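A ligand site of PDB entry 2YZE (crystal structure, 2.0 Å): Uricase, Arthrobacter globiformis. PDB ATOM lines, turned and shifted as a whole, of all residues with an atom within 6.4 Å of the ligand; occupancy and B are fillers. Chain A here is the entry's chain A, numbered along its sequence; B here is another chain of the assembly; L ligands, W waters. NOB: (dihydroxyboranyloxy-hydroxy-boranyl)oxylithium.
N of Leu 222 lies within hydrogen-bond range of OB3 of the ligand, 3.0 Å away.
The guanidinium group of Arg 180 is in hydrogen-bond range of an oxygen (OB2) of the ligand.
The side-chain hydroxyl (OG1) of Thr 67 of chain B sits at hydrogen-bond distance from an oxygen (OB4) of the ligand (3.0 Å).
ND2 of Asn 249 sits at hydrogen-bond distance from OB4 of the ligand.
N of Asn 249 sits at hydrogen-bond distance from O of Gly 277 (2.6 Å).
A ring nitrogen (NE2) of His 251 sits close to the backbone carbonyl oxygen (O) of Asn 249 (3.4 Å).
OG1 of Thr 67 of chain B is in hydrogen-bond range of NZ of Lys 22 of chain B (2.8 Å).
The side-chain amino group of Lys 22 of chain B sits close to a ring nitrogen (NE2) of His 251 (3.4 Å).
The side-chain hydroxyl (OG) of Ser 219 is in hydrogen-bond range of the backbone carbonyl oxygen (O) of Ala 221, 2.9 Å away.
The side-chain amide oxygen of Gln 223 lies close to an oxygen (OB1) of the ligand, 3.4 Å away.
Phe 163 touches the ligand (CZ to LI, 3.4 Å).
Ala 221 touches the ligand (CA to OB3, 3.8 Å).
His 251 touches the ligand (NE2 to OB4, 3.8 Å).
Val 64 of chain B touches the ligand (CG1 to OB1, 3.9 Å).
Ala 66 of chain B touches the ligand.
Hydrophobic or aromatic side chains that line the ligand: Phe 163, Leu 222 and Val 64 of chain B.
Of the 25 residues printed, 10 come within 4 Å of the ligand.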
ATOM      1  N   GLU A 162      -0.722  10.006  22.901  1.00  0.00           N
ATOM      2  CA  GLU A 162      -1.486  10.864  23.788  1.00  0.00           C
ATOM      3  C   GLU A 162      -0.553  11.503  24.807  1.00  0.00           C
ATOM      4  O   GLU A 162       0.615  11.097  24.944  1.00  0.00           O
ATOM      5  CB  GLU A 162      -2.516  10.045  24.572  1.00  0.00           C
ATOM      6  CG  GLU A 162      -3.442   9.207  23.734  1.00  0.00           C
ATOM      7  CD  GLU A 162      -4.400   8.386  24.580  1.00  0.00           C
ATOM      8  OE1 GLU A 162      -4.945   8.925  25.566  1.00  0.00           O
ATOM      9  OE2 GLU A 162      -4.629   7.207  24.243  1.00  0.00           O
ATOM     10  N   PHE A 163      -1.064  12.503  25.494  1.00  0.00           N
ATOM     11  CA  PHE A 163      -0.323  13.168  26.561  1.00  0.00           C
ATOM     12  C   PHE A 163      -1.304  13.916  27.440  1.00  0.00           C
ATOM     13  O   PHE A 163      -1.797  14.990  27.083  1.00  0.00           O
ATOM     14  CB  PHE A 163       0.731  14.136  26.033  1.00  0.00           C
ATOM     15  CG  PHE A 163       1.688  14.598  27.104  1.00  0.00           C
ATOM     16  CD1 PHE A 163       2.404  13.670  27.856  1.00  0.00           C
ATOM     17  CD2 PHE A 163       1.850  15.950  27.390  1.00  0.00           C
ATOM     18  CE1 PHE A 163       3.261  14.076  28.900  1.00  0.00           C
ATOM     19  CE2 PHE A 163       2.703  16.367  28.415  1.00  0.00           C
ATOM     20  CZ  PHE A 163       3.407  15.421  29.170  1.00  0.00           C
ATOM     21  N   LEU A 174      -0.426  24.159  28.390  1.00  0.00           N
ATOM     22  CA  LEU A 174      -0.606  23.012  27.508  1.00  0.00           C
ATOM     23  C   LEU A 174      -1.899  22.277  27.842  1.00  0.00           C
ATOM     24  O   LEU A 174      -2.171  21.993  29.009  1.00  0.00           O
ATOM     25  CB  LEU A 174       0.583  22.048  27.648  1.00  0.00           C
ATOM     26  CG  LEU A 174       0.520  20.762  26.794  1.00  0.00           C
ATOM     27  CD1 LEU A 174       0.561  21.131  25.315  1.00  0.00           C
ATOM     28  CD2 LEU A 174       1.684  19.844  27.144  1.00  0.00           C
ATOM     29  N   ARG A 180      -2.319  13.020  19.036  1.00  0.00           N
ATOM     30  CA  ARG A 180      -1.338  13.986  18.581  1.00  0.00           C
ATOM     31  C   ARG A 180      -0.278  13.264  17.775  1.00  0.00           C
ATOM     32  O   ARG A 180      -0.213  12.042  17.766  1.00  0.00           O
ATOM     33  CB  ARG A 180      -0.660  14.665  19.783  1.00  0.00           C
ATOM     34  CG  ARG A 180       0.238  13.719  20.585  1.00  0.00           C
ATOM     35  CD  ARG A 180       1.067  14.443  21.640  1.00  0.00           C
ATOM     36  NE  ARG A 180       1.977  13.510  22.304  1.00  0.00           N
ATOM     37  CZ  ARG A 180       2.896  13.852  23.199  1.00  0.00           C
ATOM     38  NH1 ARG A 180       3.048  15.122  23.555  1.00  0.00           N
ATOM     39  NH2 ARG A 180       3.680  12.922  23.722  1.00  0.00           N
ATOM     40  N   LEU A 182       3.538  12.222  17.094  1.00  0.00           N
ATOM     41  CA  LEU A 182       4.723  11.983  17.907  1.00  0.00           C
ATOM     42  C   LEU A 182       5.841  11.776  16.894  1.00  0.00           C
ATOM     43  O   LEU A 182       5.873  10.775  16.190  1.00  0.00           O
ATOM     44  CB  LEU A 182       4.564  10.722  18.767  1.00  0.00           C
ATOM     45  CG  LEU A 182       5.779  10.345  19.634  1.00  0.00           C
ATOM     46  CD1 LEU A 182       6.029  11.436  20.669  1.00  0.00           C
ATOM     47  CD2 LEU A 182       5.527   9.013  20.327  1.00  0.00           C
ATOM     48  N   SER A 219       1.602   5.242  22.655  1.00  0.00           N
ATOM     49  CA  SER A 219       2.290   6.194  23.529  1.00  0.00           C
ATOM     50  C   SER A 219       1.453   7.134  24.381  1.00  0.00           C
ATOM     51  O   SER A 219       0.584   7.853  23.877  1.00  0.00           O
ATOM     52  CB  SER A 219       3.260   7.024  22.680  1.00  0.00           C
ATOM     53  OG  SER A 219       4.027   7.875  23.513  1.00  0.00           O
ATOM     54  N   LEU A 220       1.721   7.121  25.681  1.00  0.00           N
ATOM     55  CA  LEU A 220       1.043   7.995  26.637  1.00  0.00           C
ATOM     56  C   LEU A 220       2.043   9.081  27.023  1.00  0.00           C
ATOM     57  O   LEU A 220       1.707  10.025  27.717  1.00  0.00           O
ATOM     58  CB  LEU A 220       0.623   7.213  27.882  1.00  0.00           C
ATOM     59  CG  LEU A 220      -0.364   6.070  27.635  1.00  0.00           C
ATOM     60  CD1 LEU A 220      -0.714   5.397  28.961  1.00  0.00           C
ATOM     61  CD2 LEU A 220      -1.621   6.618  26.971  1.00  0.00           C
ATOM     62  N   ALA A 221       3.268   8.921  26.545  1.00  0.00           N
ATOM     63  CA  ALA A 221       4.349   9.857  26.812  1.00  0.00           C
ATOM     64  C   ALA A 221       5.582   9.393  26.047  1.00  0.00           C
ATOM     65  O   ALA A 221       5.779   8.199  25.834  1.00  0.00           O
ATOM     66  CB  ALA A 221       4.650   9.914  28.295  1.00  0.00           C
ATOM     67  N   LEU A 222       6.406  10.341  25.606  1.00  0.00           N
ATOM     68  CA  LEU A 222       7.622   9.979  24.875  1.00  0.00           C
ATOM     69  C   LEU A 222       8.494   9.123  25.796  1.00  0.00           C
ATOM     70  O   LEU A 222       9.196   8.229  25.343  1.00  0.00           O
ATOM     71  CB  LEU A 222       8.390  11.227  24.463  1.00  0.00           C
ATOM     72  CG  LEU A 222       9.021  11.245  23.066  1.00  0.00           C
ATOM     73  CD1 LEU A 222      10.166  12.242  23.067  1.00  0.00           C
ATOM     74  CD2 LEU A 222       9.529   9.871  22.675  1.00  0.00           C
ATOM     75  N   GLN A 223       8.436   9.420  27.101  1.00  0.00           N
ATOM     76  CA  GLN A 223       9.217   8.677  28.089  1.00  0.00           C
ATOM     77  C   GLN A 223       8.856   7.194  28.039  1.00  0.00           C
ATOM     78  O   GLN A 223       9.736   6.336  28.121  1.00  0.00           O
ATOM     79  CB  GLN A 223       8.986   9.216  29.516  1.00  0.00           C
ATOM     80  CG  GLN A 223       9.651  10.567  29.790  1.00  0.00           C
ATOM     81  CD  GLN A 223       8.764  11.748  29.442  1.00  0.00           C
ATOM     82  OE1 GLN A 223       7.934  11.666  28.551  1.00  0.00           O
ATOM     83  NE2 GLN A 223       8.949  12.870  30.143  1.00  0.00           N
ATOM     84  N   ASN A 249      11.404  15.805  21.002  1.00  0.00           N
ATOM     85  CA  ASN A 249       9.974  15.718  20.706  1.00  0.00           C
ATOM     86  C   ASN A 249       9.786  16.842  19.698  1.00  0.00           C
ATOM     87  O   ASN A 249       9.603  17.997  20.081  1.00  0.00           O
ATOM     88  CB  ASN A 249       9.122  15.970  21.948  1.00  0.00           C
ATOM     89  CG  ASN A 249       7.669  15.570  21.749  1.00  0.00           C
ATOM     90  OD1 ASN A 249       7.247  15.285  20.628  1.00  0.00           O
ATOM     91  ND2 ASN A 249       6.900  15.552  22.831  1.00  0.00           N
ATOM     92  N   HIS A 251       7.931  18.937  17.709  1.00  0.00           N
ATOM     93  CA  HIS A 251       6.555  19.409  17.690  1.00  0.00           C
ATOM     94  C   HIS A 251       5.931  19.708  16.340  1.00  0.00           C
ATOM     95  O   HIS A 251       6.466  20.488  15.542  1.00  0.00           O
ATOM     96  CB  HIS A 251       6.438  20.628  18.603  1.00  0.00           C
ATOM     97  CG  HIS A 251       6.935  20.387  19.995  1.00  0.00           C
ATOM     98  ND1 HIS A 251       7.854  21.203  20.614  1.00  0.00           N
ATOM     99  CD2 HIS A 251       6.646  19.406  20.893  1.00  0.00           C
ATOM    100  CE1 HIS A 251       8.109  20.750  21.821  1.00  0.00           C
ATOM    101  NE2 HIS A 251       7.392  19.664  22.021  1.00  0.00           N
ATOM    102  N   TYR A 276      12.209  22.332  21.269  1.00  0.00           N
ATOM    103  CA  TYR A 276      11.708  20.972  21.155  1.00  0.00           C
ATOM    104  C   TYR A 276      11.903  20.261  22.485  1.00  0.00           C
ATOM    105  O   TYR A 276      12.832  20.557  23.227  1.00  0.00           O
ATOM    106  CB  TYR A 276      12.439  20.198  20.054  1.00  0.00           C
ATOM    107  CG  TYR A 276      13.951  20.280  20.138  1.00  0.00           C
ATOM    108  CD1 TYR A 276      14.635  21.383  19.614  1.00  0.00           C
ATOM    109  CD2 TYR A 276      14.703  19.281  20.759  1.00  0.00           C
ATOM    110  CE1 TYR A 276      16.016  21.494  19.707  1.00  0.00           C
ATOM    111  CE2 TYR A 276      16.095  19.380  20.859  1.00  0.00           C
ATOM    112  CZ  TYR A 276      16.745  20.488  20.325  1.00  0.00           C
ATOM    113  OH  TYR A 276      18.109  20.632  20.415  1.00  0.00           O
ATOM    114  N   GLY A 277      11.025  19.316  22.786  1.00  0.00           N
ATOM    115  CA  GLY A 277      11.195  18.571  24.016  1.00  0.00           C
ATOM    116  C   GLY A 277      12.409  17.687  23.789  1.00  0.00           C
ATOM    117  O   GLY A 277      12.685  17.271  22.662  1.00  0.00           O
ATOM    118  N   LEU A 278      13.168  17.419  24.841  1.00  0.00           N
ATOM    119  CA  LEU A 278      14.323  16.539  24.726  1.00  0.00           C
ATOM    120  C   LEU A 278      14.200  15.547  25.867  1.00  0.00           C
ATOM    121  O   LEU A 278      14.370  15.907  27.026  1.00  0.00           O
ATOM    122  CB  LEU A 278      15.626  17.327  24.853  1.00  0.00           C
ATOM    123  CG  LEU A 278      16.909  16.500  24.725  1.00  0.00           C
ATOM    124  CD1 LEU A 278      16.906  15.707  23.400  1.00  0.00           C
ATOM    125  CD2 LEU A 278      18.109  17.426  24.798  1.00  0.00           C
ATOM    126  N   ILE A 279      13.864  14.303  25.514  1.00  0.00           N
ATOM    127  CA  ILE A 279      13.689  13.253  26.509  1.00  0.00           C
ATOM    128  C   ILE A 279      14.852  12.260  26.404  1.00  0.00           C
ATOM    129  O   ILE A 279      15.126  11.732  25.321  1.00  0.00           O
ATOM    130  CB  ILE A 279      12.335  12.515  26.297  1.00  0.00           C
ATOM    131  CG1 ILE A 279      11.186  13.380  26.817  1.00  0.00           C
ATOM    132  CG2 ILE A 279      12.333  11.195  27.042  1.00  0.00           C
ATOM    133  CD1 ILE A 279      11.045  14.748  26.169  1.00  0.00           C
ATOM    134  N   TYR B  20      14.706  15.153  31.332  1.00  0.00           N
ATOM    135  CA  TYR B  20      13.871  15.594  30.232  1.00  0.00           C
ATOM    136  C   TYR B  20      13.493  17.057  30.425  1.00  0.00           C
ATOM    137  O   TYR B  20      13.521  17.581  31.533  1.00  0.00           O
ATOM    138  CB  TYR B  20      12.589  14.761  30.158  1.00  0.00           C
ATOM    139  CG  TYR B  20      11.536  15.253  31.123  1.00  0.00           C
ATOM    140  CD1 TYR B  20      11.707  15.140  32.496  1.00  0.00           C
ATOM    141  CD2 TYR B  20      10.399  15.938  30.653  1.00  0.00           C
ATOM    142  CE1 TYR B  20      10.800  15.695  33.391  1.00  0.00           C
ATOM    143  CE2 TYR B  20       9.488  16.504  31.530  1.00  0.00           C
ATOM    144  CZ  TYR B  20       9.698  16.376  32.900  1.00  0.00           C
ATOM    145  OH  TYR B  20       8.822  16.967  33.778  1.00  0.00           O
ATOM    146  N   GLY B  21      13.123  17.725  29.331  1.00  0.00           N
ATOM    147  CA  GLY B  21      12.747  19.120  29.424  1.00  0.00           C
ATOM    148  C   GLY B  21      12.646  19.759  28.050  1.00  0.00           C
ATOM    149  O   GLY B  21      12.513  19.065  27.053  1.00  0.00           O
ATOM    150  N   LYS B  22      12.696  21.087  28.012  1.00  0.00           N
ATOM    151  CA  LYS B  22      12.618  21.799  26.752  1.00  0.00           C
ATOM    152  C   LYS B  22      13.994  22.282  26.353  1.00  0.00           C
ATOM    153  O   LYS B  22      14.670  22.977  27.127  1.00  0.00           O
ATOM    154  CB  LYS B  22      11.680  23.003  26.849  1.00  0.00           C
ATOM    155  CG  LYS B  22      11.383  23.618  25.500  1.00  0.00           C
ATOM    156  CD  LYS B  22      10.453  22.709  24.679  1.00  0.00           C
ATOM    157  CE  LYS B  22       9.003  22.893  25.130  1.00  0.00           C
ATOM    158  NZ  LYS B  22       8.037  22.037  24.377  1.00  0.00           N
ATOM    159  N   ASN B  61       1.739  10.363  33.869  1.00  0.00           N
ATOM    160  CA  ASN B  61       2.382  11.676  33.844  1.00  0.00           C
ATOM    161  C   ASN B  61       2.205  12.610  35.035  1.00  0.00           C
ATOM    162  O   ASN B  61       2.500  13.805  34.925  1.00  0.00           O
ATOM    163  CB  ASN B  61       1.965  12.407  32.571  1.00  0.00           C
ATOM    164  CG  ASN B  61       2.376  11.643  31.314  1.00  0.00           C
ATOM    165  OD1 ASN B  61       3.544  11.289  31.152  1.00  0.00           O
ATOM    166  ND2 ASN B  61       1.419  11.398  30.427  1.00  0.00           N
ATOM    167  N   VAL B  64       5.261  14.465  35.606  1.00  0.00           N
ATOM    168  CA  VAL B  64       5.829  15.131  34.445  1.00  0.00           C
ATOM    169  C   VAL B  64       5.456  16.588  34.207  1.00  0.00           C
ATOM    170  O   VAL B  64       4.439  16.878  33.578  1.00  0.00           O
ATOM    171  CB  VAL B  64       5.510  14.332  33.160  1.00  0.00           C
ATOM    172  CG1 VAL B  64       6.230  14.957  31.961  1.00  0.00           C
ATOM    173  CG2 VAL B  64       5.940  12.879  33.339  1.00  0.00           C
ATOM    174  N   VAL B  65       6.271  17.504  34.717  1.00  0.00           N
ATOM    175  CA  VAL B  65       6.042  18.920  34.486  1.00  0.00           C
ATOM    176  C   VAL B  65       6.286  19.049  32.982  1.00  0.00           C
ATOM    177  O   VAL B  65       7.385  18.795  32.513  1.00  0.00           O
ATOM    178  CB  VAL B  65       7.078  19.775  35.261  1.00  0.00           C
ATOM    179  CG1 VAL B  65       6.884  21.260  34.942  1.00  0.00           C
ATOM    180  CG2 VAL B  65       6.942  19.531  36.756  1.00  0.00           C
ATOM    181  N   ALA B  66       5.249  19.417  32.218  1.00  0.00           N
ATOM    182  CA  ALA B  66       5.373  19.500  30.756  1.00  0.00           C
ATOM    183  C   ALA B  66       6.556  20.327  30.262  1.00  0.00           C
ATOM    184  O   ALA B  66       6.898  21.349  30.868  1.00  0.00           O
ATOM    185  CB  ALA B  66       4.057  20.045  30.140  1.00  0.00           C
ATOM    186  N   THR B  67       7.189  19.890  29.175  1.00  0.00           N
ATOM    187  CA  THR B  67       8.308  20.647  28.643  1.00  0.00           C
ATOM    188  C   THR B  67       7.764  22.013  28.229  1.00  0.00           C
ATOM    189  O   THR B  67       8.457  23.022  28.332  1.00  0.00           O
ATOM    190  CB  THR B  67       8.993  19.933  27.435  1.00  0.00           C
ATOM    191  OG1 THR B  67       8.135  20.005  26.282  1.00  0.00           O
ATOM    192  CG2 THR B  67       9.254  18.469  27.757  1.00  0.00           C
ATOM    193  N   ASP B  68       6.511  22.038  27.774  1.00  0.00           N
ATOM    194  CA  ASP B  68       5.894  23.303  27.373  1.00  0.00           C
ATOM    195  C   ASP B  68       5.838  24.250  28.571  1.00  0.00           C
ATOM    196  O   ASP B  68       5.989  25.467  28.432  1.00  0.00           O
ATOM    197  CB  ASP B  68       4.476  23.051  26.841  1.00  0.00           C
ATOM    198  CG  ASP B  68       3.845  24.315  26.257  1.00  0.00           C
ATOM    199  OD1 ASP B  68       4.261  24.738  25.153  1.00  0.00           O
ATOM    200  OD2 ASP B  68       2.947  24.887  26.899  1.00  0.00           O
HETATM  201  B1  NOB L   1       6.118  14.647  26.817  1.00  0.00           B
HETATM  202  B2  NOB L   1       6.088  16.966  25.667  1.00  0.00           B
HETATM  203  OB1 NOB L   1       6.955  14.875  28.115  1.00  0.00           O
HETATM  204  OB2 NOB L   1       5.358  15.550  25.794  1.00  0.00           O
HETATM  205  OB3 NOB L   1       5.910  13.264  26.155  1.00  0.00           O
HETATM  206  OB4 NOB L   1       7.515  17.317  25.044  1.00  0.00           O
HETATM  207  OB5 NOB L   1       5.310  18.155  26.364  1.00  0.00           O
HETATM  208 LI   NOB L   1       6.064  17.263  27.986  1.00  0.00          LI
HETATM  209  O   HOH W   1       3.556  18.613  23.968  1.00  0.00           O
